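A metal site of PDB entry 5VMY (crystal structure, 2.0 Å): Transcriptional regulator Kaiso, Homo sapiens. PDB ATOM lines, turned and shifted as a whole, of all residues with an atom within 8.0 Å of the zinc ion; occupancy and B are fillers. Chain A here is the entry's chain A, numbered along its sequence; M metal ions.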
ATOM      1  N   GLN A  81     -10.282   9.213 -12.881  1.00  0.00           N
ATOM      2  CA  GLN A  81     -10.552   7.994 -12.116  1.00  0.00           C
ATOM      3  C   GLN A  81     -11.558   8.210 -10.995  1.00  0.00           C
ATOM      4  O   GLN A  81     -11.398   9.113 -10.181  1.00  0.00           O
ATOM      5  CB  GLN A  81      -9.269   7.415 -11.543  1.00  0.00           C
ATOM      6  CG  GLN A  81      -9.496   6.049 -10.805  1.00  0.00           C
ATOM      7  CD  GLN A  81      -8.199   5.394 -10.362  1.00  0.00           C
ATOM      8  OE1 GLN A  81      -7.184   6.061 -10.175  1.00  0.00           O
ATOM      9  NE2 GLN A  81      -8.228   4.068 -10.202  1.00  0.00           N
ATOM     10  N   CYS A  82     -12.572   7.351 -10.974  1.00  0.00           N
ATOM     11  CA  CYS A  82     -13.568   7.343  -9.904  1.00  0.00           C
ATOM     12  C   CYS A  82     -12.943   6.826  -8.614  1.00  0.00           C
ATOM     13  O   CYS A  82     -12.381   5.718  -8.576  1.00  0.00           O
ATOM     14  CB  CYS A  82     -14.763   6.479 -10.304  1.00  0.00           C
ATOM     15  SG  CYS A  82     -15.960   6.125  -8.952  1.00  0.00           S
ATOM     16  N   LEU A  83     -13.027   7.620  -7.547  1.00  0.00           N
ATOM     17  CA  LEU A  83     -12.375   7.240  -6.300  1.00  0.00           C
ATOM     18  C   LEU A  83     -13.256   6.325  -5.454  1.00  0.00           C
ATOM     19  O   LEU A  83     -12.810   5.791  -4.462  1.00  0.00           O
ATOM     20  CB  LEU A  83     -11.976   8.482  -5.502  1.00  0.00           C
ATOM     21  CG  LEU A  83     -10.884   9.297  -6.208  1.00  0.00           C
ATOM     22  CD1 LEU A  83     -10.567  10.598  -5.502  1.00  0.00           C
ATOM     23  CD2 LEU A  83      -9.624   8.450  -6.345  1.00  0.00           C
ATOM     24  N   ALA A  84     -14.498   6.124  -5.866  1.00  0.00           N
ATOM     25  CA  ALA A  84     -15.391   5.236  -5.127  1.00  0.00           C
ATOM     26  C   ALA A  84     -15.197   3.774  -5.502  1.00  0.00           C
ATOM     27  O   ALA A  84     -15.335   2.893  -4.657  1.00  0.00           O
ATOM     28  CB  ALA A  84     -16.840   5.639  -5.344  1.00  0.00           C
ATOM     29  N   CYS A  85     -14.859   3.495  -6.764  1.00  0.00           N
ATOM     30  CA  CYS A  85     -14.722   2.096  -7.211  1.00  0.00           C
ATOM     31  C   CYS A  85     -13.457   1.842  -8.061  1.00  0.00           C
ATOM     32  O   CYS A  85     -13.127   0.694  -8.361  1.00  0.00           O
ATOM     33  CB  CYS A  85     -15.958   1.685  -7.995  1.00  0.00           C
ATOM     34  SG  CYS A  85     -15.993   2.378  -9.701  1.00  0.00           S
ATOM     35  N   GLY A  86     -12.763   2.910  -8.438  1.00  0.00           N
ATOM     36  CA  GLY A  86     -11.488   2.805  -9.139  1.00  0.00           C
ATOM     37  C   GLY A  86     -11.556   2.809 -10.658  1.00  0.00           C
ATOM     38  O   GLY A  86     -10.481   2.855 -11.343  1.00  0.00           O
ATOM     39  N   LYS A  87     -12.758   2.704 -11.213  1.00  0.00           N
ATOM     40  CA  LYS A  87     -12.923   2.723 -12.683  1.00  0.00           C
ATOM     41  C   LYS A  87     -12.402   4.004 -13.255  1.00  0.00           C
ATOM     42  O   LYS A  87     -12.564   5.059 -12.643  1.00  0.00           O
ATOM     43  CB  LYS A  87     -14.393   2.556 -13.092  1.00  0.00           C
ATOM     44  CG  LYS A  87     -14.735   1.251 -13.739  1.00  0.00           C
ATOM     45  CD  LYS A  87     -16.065   0.739 -13.235  1.00  0.00           C
ATOM     46  CE  LYS A  87     -16.234  -0.749 -13.496  1.00  0.00           C
ATOM     47  NZ  LYS A  87     -17.436  -1.291 -12.816  1.00  0.00           N
ATOM     48  N   SER A  88     -11.776   3.932 -14.428  1.00  0.00           N
ATOM     49  CA  SER A  88     -11.235   5.145 -15.088  1.00  0.00           C
ATOM     50  C   SER A  88     -11.936   5.437 -16.422  1.00  0.00           C
ATOM     51  O   SER A  88     -12.471   4.537 -17.073  1.00  0.00           O
ATOM     52  CB  SER A  88      -9.728   4.987 -15.329  1.00  0.00           C
ATOM     53  OG  SER A  88      -9.063   4.563 -14.140  1.00  0.00           O
ATOM     54  N   PHE A  89     -11.875   6.705 -16.832  1.00  0.00           N
ATOM     55  CA  PHE A  89     -12.672   7.228 -17.938  1.00  0.00           C
ATOM     56  C   PHE A  89     -11.835   8.195 -18.765  1.00  0.00           C
ATOM     57  O   PHE A  89     -10.902   8.817 -18.244  1.00  0.00           O
ATOM     58  CB  PHE A  89     -13.935   7.937 -17.398  1.00  0.00           C
ATOM     59  CG  PHE A  89     -14.756   7.042 -16.520  1.00  0.00           C
ATOM     60  CD1 PHE A  89     -15.687   6.175 -17.082  1.00  0.00           C
ATOM     61  CD2 PHE A  89     -14.549   7.011 -15.157  1.00  0.00           C
ATOM     62  CE1 PHE A  89     -16.390   5.294 -16.307  1.00  0.00           C
ATOM     63  CE2 PHE A  89     -15.265   6.133 -14.367  1.00  0.00           C
ATOM     64  CZ  PHE A  89     -16.184   5.262 -14.944  1.00  0.00           C
ATOM     65  N   MET A  95     -16.885  10.210 -16.703  1.00  0.00           N
ATOM     66  CA  MET A  95     -16.641  10.076 -15.263  1.00  0.00           C
ATOM     67  C   MET A  95     -17.863  10.587 -14.507  1.00  0.00           C
ATOM     68  O   MET A  95     -18.352   9.927 -13.588  1.00  0.00           O
ATOM     69  CB  MET A  95     -15.376  10.847 -14.841  1.00  0.00           C
ATOM     70  CG  MET A  95     -15.147  10.988 -13.310  1.00  0.00           C
ATOM     71  SD  MET A  95     -16.149  12.278 -12.463  1.00  0.00           S
ATOM     72  CE  MET A  95     -15.685  13.771 -13.359  1.00  0.00           C
ATOM     73  N   HIS A  98     -20.908   8.318 -14.846  1.00  0.00           N
ATOM     74  CA  HIS A  98     -20.705   7.110 -14.024  1.00  0.00           C
ATOM     75  C   HIS A  98     -21.016   7.377 -12.554  1.00  0.00           C
ATOM     76  O   HIS A  98     -21.774   6.644 -11.892  1.00  0.00           O
ATOM     77  CB  HIS A  98     -19.265   6.598 -14.170  1.00  0.00           C
ATOM     78  CG  HIS A  98     -18.846   5.645 -13.079  1.00  0.00           C
ATOM     79  ND1 HIS A  98     -19.159   4.307 -13.109  1.00  0.00           N
ATOM     80  CD2 HIS A  98     -18.186   5.856 -11.917  1.00  0.00           C
ATOM     81  CE1 HIS A  98     -18.681   3.715 -12.014  1.00  0.00           C
ATOM     82  NE2 HIS A  98     -18.083   4.638 -11.278  1.00  0.00           N
ATOM     83  N   ILE A  99     -20.411   8.427 -12.020  1.00  0.00           N
ATOM     84  CA  ILE A  99     -20.532   8.699 -10.593  1.00  0.00           C
ATOM     85  C   ILE A  99     -21.967   9.039 -10.224  1.00  0.00           C
ATOM     86  O   ILE A  99     -22.451   8.598  -9.174  1.00  0.00           O
ATOM     87  CB  ILE A  99     -19.548   9.807 -10.165  1.00  0.00           C
ATOM     88  CG1 ILE A  99     -18.127   9.211 -10.207  1.00  0.00           C
ATOM     89  CG2 ILE A  99     -19.843  10.261  -8.747  1.00  0.00           C
ATOM     90  CD1 ILE A  99     -17.016  10.171  -9.791  1.00  0.00           C
ATOM     91  N   LYS A 100     -22.672   9.757 -11.086  1.00  0.00           N
ATOM     92  CA  LYS A 100     -24.064  10.080 -10.783  1.00  0.00           C
ATOM     93  C   LYS A 100     -24.944   8.840 -10.891  1.00  0.00           C
ATOM     94  O   LYS A 100     -25.846   8.656 -10.076  1.00  0.00           O
ATOM     95  CB  LYS A 100     -24.586  11.176 -11.713  1.00  0.00           C
ATOM     96  CG  LYS A 100     -23.980  12.543 -11.463  1.00  0.00           C
ATOM     97  CD  LYS A 100     -24.557  13.600 -12.417  1.00  0.00           C
ATOM     98  CE  LYS A 100     -23.842  14.933 -12.293  1.00  0.00           C
ATOM     99  NZ  LYS A 100     -24.369  15.958 -13.252  1.00  0.00           N
ATOM    100  N   VAL A 102     -24.044   5.402 -10.978  1.00  0.00           N
ATOM    101  CA  VAL A 102     -23.638   4.233 -10.208  1.00  0.00           C
ATOM    102  C   VAL A 102     -23.561   4.559  -8.720  1.00  0.00           C
ATOM    103  O   VAL A 102     -23.996   3.768  -7.901  1.00  0.00           O
ATOM    104  CB  VAL A 102     -22.272   3.688 -10.709  1.00  0.00           C
ATOM    105  CG1 VAL A 102     -21.841   2.493  -9.912  1.00  0.00           C
ATOM    106  CG2 VAL A 102     -22.364   3.353 -12.206  1.00  0.00           C
ATOM    107  N   HIS A 103     -23.033   5.727  -8.377  1.00  0.00           N
ATOM    108  CA  HIS A 103     -22.794   6.056  -6.968  1.00  0.00           C
ATOM    109  C   HIS A 103     -23.799   7.079  -6.410  1.00  0.00           C
ATOM    110  O   HIS A 103     -23.792   7.385  -5.198  1.00  0.00           O
ATOM    111  CB  HIS A 103     -21.345   6.554  -6.824  1.00  0.00           C
ATOM    112  CG  HIS A 103     -20.323   5.533  -7.212  1.00  0.00           C
ATOM    113  ND1 HIS A 103     -20.236   4.320  -6.574  1.00  0.00           N
ATOM    114  CD2 HIS A 103     -19.379   5.521  -8.189  1.00  0.00           C
ATOM    115  CE1 HIS A 103     -19.270   3.604  -7.133  1.00  0.00           C
ATOM    116  NE2 HIS A 103     -18.741   4.308  -8.107  1.00  0.00           N
ATOM    117  N   LEU A 113     -14.518  13.240  -5.383  1.00  0.00           N
ATOM    118  CA  LEU A 113     -15.020  11.939  -5.862  1.00  0.00           C
ATOM    119  C   LEU A 113     -14.209  11.373  -7.020  1.00  0.00           C
ATOM    120  O   LEU A 113     -14.389  10.196  -7.365  1.00  0.00           O
ATOM    121  CB  LEU A 113     -16.473  12.070  -6.303  1.00  0.00           C
ATOM    122  CG  LEU A 113     -17.416  12.456  -5.150  1.00  0.00           C
ATOM    123  CD1 LEU A 113     -18.835  12.549  -5.647  1.00  0.00           C
ATOM    124  CD2 LEU A 113     -17.295  11.452  -4.018  1.00  0.00           C
HETATM  125 ZN    ZN M   1     -17.164   4.301  -9.509  1.00  0.00          ZN
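The zinc ion is bound by a ring nitrogen (NE2) of His 98 (2.0 Å), a ring nitrogen (NE2) of His 103 (2.1 Å), the side-chain sulfur (SG) of Cys 82 (2.3 Å) and the side-chain sulfur (SG) of Cys 85 (2.3 Å). The zinc ion has four donor atoms within binding distance.
The backbone NH of Ala 84 lies close to the side-chain sulfur of Cys 82 (3.4 Å). SG of Cys 85 sits close to N of Lys 87 (3.6 Å). N of Cys 82 is in hydrogen-bond range of O of Lys 87, 2.8 Å away.
Four residues have an atom within 4 Å of the zinc ion: Cys 82, Cys 85, His 98 and His 103.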
